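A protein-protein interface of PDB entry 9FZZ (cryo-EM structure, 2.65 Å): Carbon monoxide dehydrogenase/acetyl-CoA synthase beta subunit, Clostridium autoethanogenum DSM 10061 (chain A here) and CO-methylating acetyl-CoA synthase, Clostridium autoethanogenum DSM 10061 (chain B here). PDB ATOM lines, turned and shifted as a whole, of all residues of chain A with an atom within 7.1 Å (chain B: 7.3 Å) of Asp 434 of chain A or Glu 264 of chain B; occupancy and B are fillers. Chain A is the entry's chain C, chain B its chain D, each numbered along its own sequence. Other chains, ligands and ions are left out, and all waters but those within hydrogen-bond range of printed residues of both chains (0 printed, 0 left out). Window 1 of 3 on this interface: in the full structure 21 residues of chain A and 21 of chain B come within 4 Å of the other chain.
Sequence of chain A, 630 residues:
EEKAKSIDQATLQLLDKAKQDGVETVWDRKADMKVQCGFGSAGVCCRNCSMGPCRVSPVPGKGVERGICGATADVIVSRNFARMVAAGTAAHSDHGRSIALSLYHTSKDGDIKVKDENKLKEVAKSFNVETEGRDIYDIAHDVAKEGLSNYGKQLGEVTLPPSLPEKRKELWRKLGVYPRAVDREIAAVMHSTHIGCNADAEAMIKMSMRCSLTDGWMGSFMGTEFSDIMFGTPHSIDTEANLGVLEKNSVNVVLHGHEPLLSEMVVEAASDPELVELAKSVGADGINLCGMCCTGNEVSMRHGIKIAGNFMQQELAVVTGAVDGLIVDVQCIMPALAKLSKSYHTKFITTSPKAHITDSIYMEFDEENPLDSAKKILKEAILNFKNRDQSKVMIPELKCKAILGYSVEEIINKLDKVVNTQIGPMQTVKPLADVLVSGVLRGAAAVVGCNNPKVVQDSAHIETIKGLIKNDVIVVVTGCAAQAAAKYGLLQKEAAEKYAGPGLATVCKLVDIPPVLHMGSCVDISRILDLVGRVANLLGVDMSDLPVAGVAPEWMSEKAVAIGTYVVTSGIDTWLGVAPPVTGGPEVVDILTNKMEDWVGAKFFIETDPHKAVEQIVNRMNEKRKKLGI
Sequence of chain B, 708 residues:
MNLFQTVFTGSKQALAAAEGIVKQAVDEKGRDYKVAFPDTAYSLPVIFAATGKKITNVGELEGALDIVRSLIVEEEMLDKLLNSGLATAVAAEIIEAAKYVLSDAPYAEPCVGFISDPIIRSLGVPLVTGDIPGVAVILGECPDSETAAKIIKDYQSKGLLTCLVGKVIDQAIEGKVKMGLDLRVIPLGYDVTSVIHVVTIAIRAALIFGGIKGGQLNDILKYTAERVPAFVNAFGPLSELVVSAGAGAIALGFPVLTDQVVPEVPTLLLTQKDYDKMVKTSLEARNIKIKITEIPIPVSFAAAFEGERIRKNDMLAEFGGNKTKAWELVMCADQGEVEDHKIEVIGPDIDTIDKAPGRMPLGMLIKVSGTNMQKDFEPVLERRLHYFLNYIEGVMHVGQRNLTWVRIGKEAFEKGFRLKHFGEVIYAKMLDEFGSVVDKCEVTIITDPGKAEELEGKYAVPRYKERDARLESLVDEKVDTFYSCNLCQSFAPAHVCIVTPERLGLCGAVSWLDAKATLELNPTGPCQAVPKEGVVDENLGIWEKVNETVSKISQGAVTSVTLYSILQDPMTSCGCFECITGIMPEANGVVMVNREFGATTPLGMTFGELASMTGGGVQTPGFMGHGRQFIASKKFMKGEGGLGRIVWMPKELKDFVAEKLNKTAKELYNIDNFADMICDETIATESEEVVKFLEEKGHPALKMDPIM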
ATOM      1  N   ILE A 423      24.773  31.028   0.220  1.00  0.00           N
ATOM      2  CA  ILE A 423      24.913  29.871   1.101  1.00  0.00           C
ATOM      3  C   ILE A 423      26.342  29.333   1.080  1.00  0.00           C
ATOM      4  O   ILE A 423      27.021  29.307   2.106  1.00  0.00           O
ATOM      5  CB  ILE A 423      23.890  28.767   0.743  1.00  0.00           C
ATOM      6  CG1 ILE A 423      22.457  29.310   0.842  1.00  0.00           C
ATOM      7  CG2 ILE A 423      24.085  27.546   1.659  1.00  0.00           C
ATOM      8  CD1 ILE A 423      21.405  28.348   0.293  1.00  0.00           C
ATOM      9  N   GLY A 424      26.808  28.890  -0.083  1.00  0.00           N
ATOM     10  CA  GLY A 424      28.113  28.288  -0.216  1.00  0.00           C
ATOM     11  C   GLY A 424      28.181  26.937   0.468  1.00  0.00           C
ATOM     12  O   GLY A 424      27.154  26.341   0.801  1.00  0.00           O
ATOM     13  N   VAL A 429      32.880  19.396  -3.196  1.00  0.00           N
ATOM     14  CA  VAL A 429      32.080  18.372  -3.858  1.00  0.00           C
ATOM     15  C   VAL A 429      30.694  18.360  -3.225  1.00  0.00           C
ATOM     16  O   VAL A 429      29.884  17.462  -3.475  1.00  0.00           O
ATOM     17  CB  VAL A 429      32.761  16.993  -3.758  1.00  0.00           C
ATOM     18  CG1 VAL A 429      34.144  17.043  -4.416  1.00  0.00           C
ATOM     19  CG2 VAL A 429      32.872  16.531  -2.287  1.00  0.00           C
ATOM     20  N   LYS A 430      30.393  19.396  -2.441  1.00  0.00           N
ATOM     21  CA  LYS A 430      29.137  19.412  -1.699  1.00  0.00           C
ATOM     22  C   LYS A 430      27.896  19.300  -2.574  1.00  0.00           C
ATOM     23  O   LYS A 430      26.968  18.580  -2.173  1.00  0.00           O
ATOM     24  CB  LYS A 430      29.057  20.666  -0.828  1.00  0.00           C
ATOM     25  CG  LYS A 430      27.853  20.654   0.108  1.00  0.00           C
ATOM     26  CD  LYS A 430      27.890  21.856   1.042  1.00  0.00           C
ATOM     27  CE  LYS A 430      26.810  21.743   2.120  1.00  0.00           C
ATOM     28  NZ  LYS A 430      25.436  21.676   1.513  1.00  0.00           N
ATOM     29  N   PRO A 431      27.777  19.978  -3.724  1.00  0.00           N
ATOM     30  CA  PRO A 431      26.577  19.746  -4.560  1.00  0.00           C
ATOM     31  C   PRO A 431      26.395  18.288  -4.973  1.00  0.00           C
ATOM     32  O   PRO A 431      25.262  17.784  -4.975  1.00  0.00           O
ATOM     33  CB  PRO A 431      26.790  20.682  -5.763  1.00  0.00           C
ATOM     34  CG  PRO A 431      27.721  21.772  -5.249  1.00  0.00           C
ATOM     35  CD  PRO A 431      28.618  21.077  -4.233  1.00  0.00           C
ATOM     36  N   LEU A 432      27.487  17.592  -5.300  1.00  0.00           N
ATOM     37  CA  LEU A 432      27.411  16.174  -5.650  1.00  0.00           C
ATOM     38  C   LEU A 432      26.978  15.338  -4.452  1.00  0.00           C
ATOM     39  O   LEU A 432      26.117  14.457  -4.572  1.00  0.00           O
ATOM     40  CB  LEU A 432      28.766  15.694  -6.190  1.00  0.00           C
ATOM     41  CG  LEU A 432      28.892  14.188  -6.490  1.00  0.00           C
ATOM     42  CD1 LEU A 432      27.889  13.741  -7.575  1.00  0.00           C
ATOM     43  CD2 LEU A 432      30.334  13.831  -6.888  1.00  0.00           C
ATOM     44  N   ALA A 433      27.536  15.634  -3.282  1.00  0.00           N
ATOM     45  CA  ALA A 433      27.120  14.946  -2.067  1.00  0.00           C
ATOM     46  C   ALA A 433      25.646  15.197  -1.793  1.00  0.00           C
ATOM     47  O   ALA A 433      24.924  14.289  -1.373  1.00  0.00           O
ATOM     48  CB  ALA A 433      27.983  15.383  -0.881  1.00  0.00           C
ATOM     49  N   ASP A 434      25.168  16.417  -2.050  1.00  0.00           N
ATOM     50  CA  ASP A 434      23.765  16.746  -1.818  1.00  0.00           C
ATOM     51  C   ASP A 434      22.848  15.963  -2.743  1.00  0.00           C
ATOM     52  O   ASP A 434      21.859  15.376  -2.294  1.00  0.00           O
ATOM     53  CB  ASP A 434      23.520  18.244  -2.016  1.00  0.00           C
ATOM     54  CG  ASP A 434      24.189  19.099  -0.966  1.00  0.00           C
ATOM     55  OD1 ASP A 434      24.318  18.622   0.182  1.00  0.00           O
ATOM     56  OD2 ASP A 434      24.585  20.239  -1.276  1.00  0.00           O
ATOM     57  N   VAL A 435      23.177  15.904  -4.033  1.00  0.00           N
ATOM     58  CA  VAL A 435      22.302  15.178  -4.956  1.00  0.00           C
ATOM     59  C   VAL A 435      22.317  13.686  -4.633  1.00  0.00           C
ATOM     60  O   VAL A 435      21.281  13.018  -4.726  1.00  0.00           O
ATOM     61  CB  VAL A 435      22.668  15.452  -6.429  1.00  0.00           C
ATOM     62  CG1 VAL A 435      22.541  16.947  -6.743  1.00  0.00           C
ATOM     63  CG2 VAL A 435      24.056  14.947  -6.765  1.00  0.00           C
ATOM     64  N   LEU A 436      23.462  13.154  -4.192  1.00  0.00           N
ATOM     65  CA  LEU A 436      23.521  11.743  -3.800  1.00  0.00           C
ATOM     66  C   LEU A 436      22.721  11.480  -2.527  1.00  0.00           C
ATOM     67  O   LEU A 436      21.982  10.494  -2.449  1.00  0.00           O
ATOM     68  CB  LEU A 436      24.973  11.296  -3.610  1.00  0.00           C
ATOM     69  CG  LEU A 436      25.780  11.130  -4.908  1.00  0.00           C
ATOM     70  CD1 LEU A 436      27.243  10.836  -4.576  1.00  0.00           C
ATOM     71  CD2 LEU A 436      25.185  10.035  -5.831  1.00  0.00           C
ATOM     72  N   VAL A 437      22.840  12.354  -1.526  1.00  0.00           N
ATOM     73  CA  VAL A 437      22.146  12.125  -0.262  1.00  0.00           C
ATOM     74  C   VAL A 437      20.642  12.278  -0.449  1.00  0.00           C
ATOM     75  O   VAL A 437      19.856  11.500   0.103  1.00  0.00           O
ATOM     76  CB  VAL A 437      22.693  13.080   0.819  1.00  0.00           C
ATOM     77  CG1 VAL A 437      21.719  13.195   2.007  1.00  0.00           C
ATOM     78  CG2 VAL A 437      24.082  12.611   1.290  1.00  0.00           C
ATOM     79  N   SER A 438      20.210  13.288  -1.206  1.00  0.00           N
ATOM     80  CA  SER A 438      18.776  13.502  -1.382  1.00  0.00           C
ATOM     81  C   SER A 438      18.117  12.370  -2.167  1.00  0.00           C
ATOM     82  O   SER A 438      16.907  12.172  -2.031  1.00  0.00           O
ATOM     83  CB  SER A 438      18.502  14.857  -2.064  1.00  0.00           C
ATOM     84  OG  SER A 438      18.915  14.850  -3.425  1.00  0.00           O
ATOM     85  N   GLY A 439      18.879  11.600  -2.942  1.00  0.00           N
ATOM     86  CA  GLY A 439      18.297  10.556  -3.753  1.00  0.00           C
ATOM     87  C   GLY A 439      17.937  10.975  -5.163  1.00  0.00           C
ATOM     88  O   GLY A 439      17.430  10.140  -5.921  1.00  0.00           O
ATOM     89  N   VAL A 440      18.181  12.232  -5.537  1.00  0.00           N
ATOM     90  CA  VAL A 440      17.985  12.647  -6.925  1.00  0.00           C
ATOM     91  C   VAL A 440      18.889  11.823  -7.828  1.00  0.00           C
ATOM     92  O   VAL A 440      18.486  11.391  -8.915  1.00  0.00           O
ATOM     93  CB  VAL A 440      18.224  14.161  -7.080  1.00  0.00           C
ATOM     94  CG1 VAL A 440      18.202  14.577  -8.557  1.00  0.00           C
ATOM     95  CG2 VAL A 440      17.159  14.952  -6.295  1.00  0.00           C
ATOM     96  N   LEU A 441      20.128  11.603  -7.402  1.00  0.00           N
ATOM     97  CA  LEU A 441      21.009  10.609  -8.000  1.00  0.00           C
ATOM     98  C   LEU A 441      21.057   9.398  -7.073  1.00  0.00           C
ATOM     99  O   LEU A 441      21.258   9.540  -5.862  1.00  0.00           O
ATOM    100  CB  LEU A 441      22.417  11.162  -8.238  1.00  0.00           C
ATOM    101  CG  LEU A 441      22.559  12.210  -9.355  1.00  0.00           C
ATOM    102  CD1 LEU A 441      24.052  12.497  -9.553  1.00  0.00           C
ATOM    103  CD2 LEU A 441      21.896  11.808 -10.685  1.00  0.00           C
ATOM    104  N   VAL A 535      33.971  12.921  -1.243  1.00  0.00           N
ATOM    105  CA  VAL A 535      32.569  12.787  -0.865  1.00  0.00           C
ATOM    106  C   VAL A 535      32.469  12.154   0.510  1.00  0.00           C
ATOM    107  O   VAL A 535      31.791  12.667   1.408  1.00  0.00           O
ATOM    108  CB  VAL A 535      31.807  11.980  -1.928  1.00  0.00           C
ATOM    109  CG1 VAL A 535      30.374  11.719  -1.472  1.00  0.00           C
ATOM    110  CG2 VAL A 535      31.832  12.725  -3.255  1.00  0.00           C
ATOM    111  N   LEU A 538      33.387  14.495   3.142  1.00  0.00           N
ATOM    112  CA  LEU A 538      32.393  15.533   3.368  1.00  0.00           C
ATOM    113  C   LEU A 538      31.226  15.014   4.186  1.00  0.00           C
ATOM    114  O   LEU A 538      30.626  15.774   4.951  1.00  0.00           O
ATOM    115  CB  LEU A 538      31.911  16.108   2.031  1.00  0.00           C
ATOM    116  CG  LEU A 538      31.159  17.447   2.118  1.00  0.00           C
ATOM    117  CD1 LEU A 538      31.795  18.419   3.121  1.00  0.00           C
ATOM    118  CD2 LEU A 538      31.115  18.096   0.746  1.00  0.00           C
ATOM    119  N   LEU A 539      30.934  13.720   4.093  1.00  0.00           N
ATOM    120  CA  LEU A 539      29.805  13.126   4.791  1.00  0.00           C
ATOM    121  C   LEU A 539      30.206  12.467   6.104  1.00  0.00           C
ATOM    122  O   LEU A 539      29.331  11.982   6.829  1.00  0.00           O
ATOM    123  CB  LEU A 539      29.103  12.102   3.888  1.00  0.00           C
ATOM    124  CG  LEU A 539      28.437  12.679   2.627  1.00  0.00           C
ATOM    125  CD1 LEU A 539      27.840  11.559   1.787  1.00  0.00           C
ATOM    126  CD2 LEU A 539      27.361  13.726   2.982  1.00  0.00           C
ATOM    127  N   LEU B   3      14.450  11.846   1.975  1.00  0.00           N
ATOM    128  CA  LEU B   3      13.609  12.850   1.327  1.00  0.00           C
ATOM    129  C   LEU B   3      12.415  12.223   0.623  1.00  0.00           C
ATOM    130  O   LEU B   3      11.273  12.667   0.798  1.00  0.00           O
ATOM    131  CB  LEU B   3      14.447  13.660   0.330  1.00  0.00           C
ATOM    132  CG  LEU B   3      13.669  14.723  -0.466  1.00  0.00           C
ATOM    133  CD1 LEU B   3      13.091  15.778   0.482  1.00  0.00           C
ATOM    134  CD2 LEU B   3      14.551  15.368  -1.541  1.00  0.00           C
ATOM    135  N   THR B 258      14.457  27.112   3.288  1.00  0.00           N
ATOM    136  CA  THR B 258      14.038  26.836   4.653  1.00  0.00           C
ATOM    137  C   THR B 258      15.199  27.123   5.593  1.00  0.00           C
ATOM    138  O   THR B 258      16.360  27.152   5.183  1.00  0.00           O
ATOM    139  CB  THR B 258      13.552  25.382   4.810  1.00  0.00           C
ATOM    140  OG1 THR B 258      13.052  25.161   6.136  1.00  0.00           O
ATOM    141  CG2 THR B 258      14.683  24.386   4.528  1.00  0.00           C
ATOM    142  N   GLN B 260      15.489  25.072   8.196  1.00  0.00           N
ATOM    143  CA  GLN B 260      15.633  23.763   8.803  1.00  0.00           C
ATOM    144  C   GLN B 260      16.652  22.930   8.035  1.00  0.00           C
ATOM    145  O   GLN B 260      16.903  23.147   6.848  1.00  0.00           O
ATOM    146  CB  GLN B 260      14.282  23.035   8.821  1.00  0.00           C
ATOM    147  CG  GLN B 260      13.175  23.839   9.511  1.00  0.00           C
ATOM    148  CD  GLN B 260      13.434  23.994  10.995  1.00  0.00           C
ATOM    149  OE1 GLN B 260      13.574  23.008  11.705  1.00  0.00           O
ATOM    150  NE2 GLN B 260      13.514  25.238  11.472  1.00  0.00           N
ATOM    151  N   VAL B 261      17.235  21.961   8.740  1.00  0.00           N
ATOM    152  CA  VAL B 261      18.147  21.009   8.119  1.00  0.00           C
ATOM    153  C   VAL B 261      17.321  20.035   7.288  1.00  0.00           C
ATOM    154  O   VAL B 261      16.436  19.344   7.816  1.00  0.00           O
ATOM    155  CB  VAL B 261      18.987  20.272   9.171  1.00  0.00           C
ATOM    156  CG1 VAL B 261      19.921  19.253   8.500  1.00  0.00           C
ATOM    157  CG2 VAL B 261      19.797  21.268   9.996  1.00  0.00           C
ATOM    158  N   VAL B 262      17.580  19.999   5.992  1.00  0.00           N
ATOM    159  CA  VAL B 262      16.850  19.141   5.062  1.00  0.00           C
ATOM    160  C   VAL B 262      17.835  18.510   4.096  1.00  0.00           C
ATOM    161  O   VAL B 262      18.980  18.962   3.962  1.00  0.00           O
ATOM    162  CB  VAL B 262      15.773  19.921   4.278  1.00  0.00           C
ATOM    163  CG1 VAL B 262      14.721  20.497   5.227  1.00  0.00           C
ATOM    164  CG2 VAL B 262      16.415  21.026   3.440  1.00  0.00           C
ATOM    165  N   PRO B 263      17.414  17.435   3.403  1.00  0.00           N
ATOM    166  CA  PRO B 263      18.246  16.882   2.319  1.00  0.00           C
ATOM    167  C   PRO B 263      18.259  17.800   1.112  1.00  0.00           C
ATOM    168  O   PRO B 263      17.461  17.666   0.178  1.00  0.00           O
ATOM    169  CB  PRO B 263      17.590  15.529   2.005  1.00  0.00           C
ATOM    170  CG  PRO B 263      16.798  15.179   3.253  1.00  0.00           C
ATOM    171  CD  PRO B 263      16.332  16.514   3.799  1.00  0.00           C
ATOM    172  N   GLU B 264      19.188  18.751   1.139  1.00  0.00           N
ATOM    173  CA  GLU B 264      19.244  19.795   0.134  1.00  0.00           C
ATOM    174  C   GLU B 264      19.392  19.231  -1.277  1.00  0.00           C
ATOM    175  O   GLU B 264      20.121  18.261  -1.509  1.00  0.00           O
ATOM    176  CB  GLU B 264      20.404  20.738   0.431  1.00  0.00           C
ATOM    177  CG  GLU B 264      20.089  21.768   1.508  1.00  0.00           C
ATOM    178  CD  GLU B 264      21.255  22.710   1.712  1.00  0.00           C
ATOM    179  OE1 GLU B 264      22.338  22.223   2.080  1.00  0.00           O
ATOM    180  OE2 GLU B 264      21.100  23.923   1.466  1.00  0.00           O
ATOM    181  N   VAL B 265      18.677  19.848  -2.210  1.00  0.00           N
ATOM    182  CA  VAL B 265      18.794  19.593  -3.636  1.00  0.00           C
ATOM    183  C   VAL B 265      19.230  20.893  -4.308  1.00  0.00           C
ATOM    184  O   VAL B 265      18.515  21.896  -4.220  1.00  0.00           O
ATOM    185  CB  VAL B 265      17.463  19.094  -4.231  1.00  0.00           C
ATOM    186  CG1 VAL B 265      17.604  18.866  -5.738  1.00  0.00           C
ATOM    187  CG2 VAL B 265      16.994  17.823  -3.500  1.00  0.00           C
ATOM    188  N   PRO B 266      20.357  20.925  -5.028  1.00  0.00           N
ATOM    189  CA  PRO B 266      20.831  22.204  -5.590  1.00  0.00           C
ATOM    190  C   PRO B 266      19.775  22.871  -6.464  1.00  0.00           C
ATOM    191  O   PRO B 266      19.079  22.224  -7.249  1.00  0.00           O
ATOM    192  CB  PRO B 266      22.078  21.805  -6.391  1.00  0.00           C
ATOM    193  CG  PRO B 266      22.596  20.560  -5.693  1.00  0.00           C
ATOM    194  CD  PRO B 266      21.335  19.836  -5.224  1.00  0.00           C
ATOM    195  N   THR B 267      19.638  24.188  -6.268  1.00  0.00           N
ATOM    196  CA  THR B 267      18.724  25.070  -6.989  1.00  0.00           C
ATOM    197  C   THR B 267      17.243  24.805  -6.686  1.00  0.00           C
ATOM    198  O   THR B 267      16.388  25.588  -7.105  1.00  0.00           O
ATOM    199  CB  THR B 267      18.948  25.005  -8.517  1.00  0.00           C
ATOM    200  OG1 THR B 267      18.356  23.824  -9.076  1.00  0.00           O
ATOM    201  CG2 THR B 267      20.436  25.041  -8.867  1.00  0.00           C
ATOM    202  N   LEU B 268      16.922  23.762  -5.920  1.00  0.00           N
ATOM    203  CA  LEU B 268      15.529  23.403  -5.664  1.00  0.00           C
ATOM    204  C   LEU B 268      15.158  23.416  -4.188  1.00  0.00           C
ATOM    205  O   LEU B 268      14.135  24.003  -3.821  1.00  0.00           O
ATOM    206  CB  LEU B 268      15.220  22.019  -6.276  1.00  0.00           C
ATOM    207  CG  LEU B 268      15.387  21.933  -7.806  1.00  0.00           C
ATOM    208  CD1 LEU B 268      15.026  20.530  -8.311  1.00  0.00           C
ATOM    209  CD2 LEU B 268      14.549  22.992  -8.518  1.00  0.00           C
ATOM    210  N   LEU B 269      15.949  22.788  -3.327  1.00  0.00           N
ATOM    211  CA  LEU B 269      15.668  22.723  -1.898  1.00  0.00           C
ATOM    212  C   LEU B 269      16.939  23.149  -1.179  1.00  0.00           C
ATOM    213  O   LEU B 269      17.967  22.469  -1.273  1.00  0.00           O
ATOM    214  CB  LEU B 269      15.226  21.314  -1.502  1.00  0.00           C
ATOM    215  CG  LEU B 269      14.840  21.115  -0.035  1.00  0.00           C
ATOM    216  CD1 LEU B 269      13.701  22.042   0.367  1.00  0.00           C
ATOM    217  CD2 LEU B 269      14.463  19.654   0.183  1.00  0.00           C
ATOM    218  N   LEU B 270      16.879  24.285  -0.488  1.00  0.00           N
ATOM    219  CA  LEU B 270      18.055  24.907   0.100  1.00  0.00           C
ATOM    220  C   LEU B 270      17.806  25.282   1.553  1.00  0.00           C
ATOM    221  O   LEU B 270      16.718  25.737   1.912  1.00  0.00           O
ATOM    222  CB  LEU B 270      18.467  26.162  -0.682  1.00  0.00           C
ATOM    223  CG  LEU B 270      18.662  26.006  -2.197  1.00  0.00           C
ATOM    224  CD1 LEU B 270      18.907  27.378  -2.826  1.00  0.00           C
ATOM    225  CD2 LEU B 270      19.806  25.042  -2.518  1.00  0.00           C
ATOM    226  N   THR B 271      18.843  25.128   2.370  1.00  0.00           N
ATOM    227  CA  THR B 271      18.801  25.504   3.773  1.00  0.00           C
ATOM    228  C   THR B 271      19.584  26.796   3.959  1.00  0.00           C
ATOM    229  O   THR B 271      20.738  26.894   3.528  1.00  0.00           O
ATOM    230  CB  THR B 271      19.399  24.410   4.670  1.00  0.00           C
ATOM    231  OG1 THR B 271      18.546  23.258   4.702  1.00  0.00           O
ATOM    232  CG2 THR B 271      19.592  24.928   6.101  1.00  0.00           C
ATOM    233  N   GLN B 272      18.948  27.784   4.587  1.00  0.00           N
ATOM    234  CA  GLN B 272      19.587  29.056   4.911  1.00  0.00           C
ATOM    235  C   GLN B 272      19.144  29.397   6.330  1.00  0.00           C
ATOM    236  O   GLN B 272      18.002  29.816   6.545  1.00  0.00           O
ATOM    237  CB  GLN B 272      19.195  30.149   3.914  1.00  0.00           C
ATOM    238  CG  GLN B 272      19.747  31.540   4.270  1.00  0.00           C
ATOM    239  CD  GLN B 272      21.274  31.540   4.354  1.00  0.00           C
ATOM    240  OE1 GLN B 272      21.836  31.390   5.430  1.00  0.00           O
ATOM    241  NE2 GLN B 272      21.945  31.689   3.209  1.00  0.00           N
ATOM    242  N   LYS B 273      20.035  29.174   7.301  1.00  0.00           N
ATOM    243  CA  LYS B 273      19.721  29.503   8.689  1.00  0.00           C
ATOM    244  C   LYS B 273      19.777  31.001   8.961  1.00  0.00           C
ATOM    245  O   LYS B 273      18.990  31.507   9.768  1.00  0.00           O
ATOM    246  CB  LYS B 273      20.673  28.780   9.649  1.00  0.00           C
ATOM    247  CG  LYS B 273      20.087  27.488  10.252  1.00  0.00           C
ATOM    248  CD  LYS B 273      20.297  26.278   9.329  1.00  0.00           C
ATOM    249  CE  LYS B 273      21.792  25.914   9.247  1.00  0.00           C
ATOM    250  NZ  LYS B 273      22.036  24.656   8.469  1.00  0.00           N
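CD1 of Ile 423 of chain A touches CB of Leu 270 of chain B, 3.8 Å away.
Ile 423 of chain A touches Thr 271 of chain B (CD1 to O, 3.6 Å).
NE2 of Gln 272 of chain B touches CG1 of Ile 423 of chain A, at 3.4 Å.
Pro 431 of chain A touches Pro 266 of chain B.
CD of Pro 266 of chain B touches CG1 of Val 435 of chain A, at 3.5 Å.
Leu 3 of chain B touches Ser 438 of chain A (CB to O, 3.7 Å).
Ser 438 of chain A touches Pro 263 of chain B.
Glu 264 of chain B touches Ser 438 of chain A.
Ser 438 of chain A touches Val 265 of chain B (OG to CG2, 3.5 Å).
CG2 of Val 440 of chain A touches CG1 of Val 265 of chain B, at 3.98 Å.
The backbone carbonyl oxygen (O) of Gln 260 of chain B sits at hydrogen-bond distance from the side-chain hydroxyl (OG1) of Thr 271 of chain B (2.7 Å).
The side-chain amino group of Lys 430 of chain A is in salt-bridge range of the side-chain carboxylate of Asp 434 of chain A, at 3.3 Å.
The backbone carbonyl oxygen of Asp 434 of chain A sits at hydrogen-bond distance from the side-chain hydroxyl of Ser 438 of chain A, 3.2 Å away.
The side-chain hydroxyl (OG) of Ser 438 of chain A lies within hydrogen-bond range of the backbone carbonyl oxygen (O) of Val 435 of chain A, 3.3 Å away.
The backbone NH (N) of Val 440 of chain A sits at hydrogen-bond distance from the backbone carbonyl oxygen (O) of Val 435 of chain A (3.3 Å).
The backbone carbonyl oxygen (O) of Val 435 of chain A lies within hydrogen-bond range of the backbone NH (N) of Leu 441 of chain A (3.2 Å).
Of the 16 printed residues of chain B, 8 touch a printed residue of chain A.
Printed residues of chain B that touch a printed residue of chain A: Leu 3, Pro 263, Glu 264, Val 265, Pro 266, Leu 270, Thr 271 and Gln 272.
Hydrophobic or aromatic side chains of chain B within 4 Å of the printed part of chain A: Leu 3, Val 265, Pro 266 and Leu 270.
Printed residues of chain A that touch a printed residue of chain B: Ile 423, Lys 430, Pro 431, Asp 434, Val 435, Ser 438 and Val 440.
Hydrophobic or aromatic side chains of chain A that line the printed part of chain B: Ile 423, Val 435 and Val 440.
Among the printed residues, Asp or Glu carboxylates within 4 Å of a Lys or Arg side-chain nitrogen of the other chain: Lys 430 of chain A with Glu 264 of chain B (3.2 Å).
The side-chain amino group (NZ) of Lys 430 of chain A lies within salt-bridge range of the side-chain carboxylate (OE1) of Glu 264 of chain B.
The backbone carbonyl oxygen (O) of Asp 434 of chain A lies close to the backbone carbonyl oxygen (O) of Glu 264 of chain B, 3.5 Å away.
Of the printed residues of chain B, Ile 423 of chain A touches Leu 270, Thr 271 and Gln 272.
Of the printed residues of chain B, Pro 431 of chain A touches Pro 266.
Asp 434 of chain A touches one residue of chain B.
Printed residues of chain B within 4 Å of Ser 438 of chain A: Leu 3 (3.7 Å), Pro 263 (3.7 Å), Glu 264 (3.8 Å) and Val 265 (3.5 Å).
Printed residues of chain A within 4 Å of Glu 264 of chain B: Lys 430 (3.2 Å), Asp 434 (3.4 Å) and Ser 438 (3.8 Å).
The nearest residue of chain B that does not touch Asp 434 of chain A is Pro 266 of chain B (4.2 Å).
The nearest printed residue of chain A that does not touch Glu 264 of chain B is Ile 423 of chain A (4.6 Å).
The nearest printed residue of chain B that does not touch Val 435 of chain A is Glu 264 of chain B (4.6 Å).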
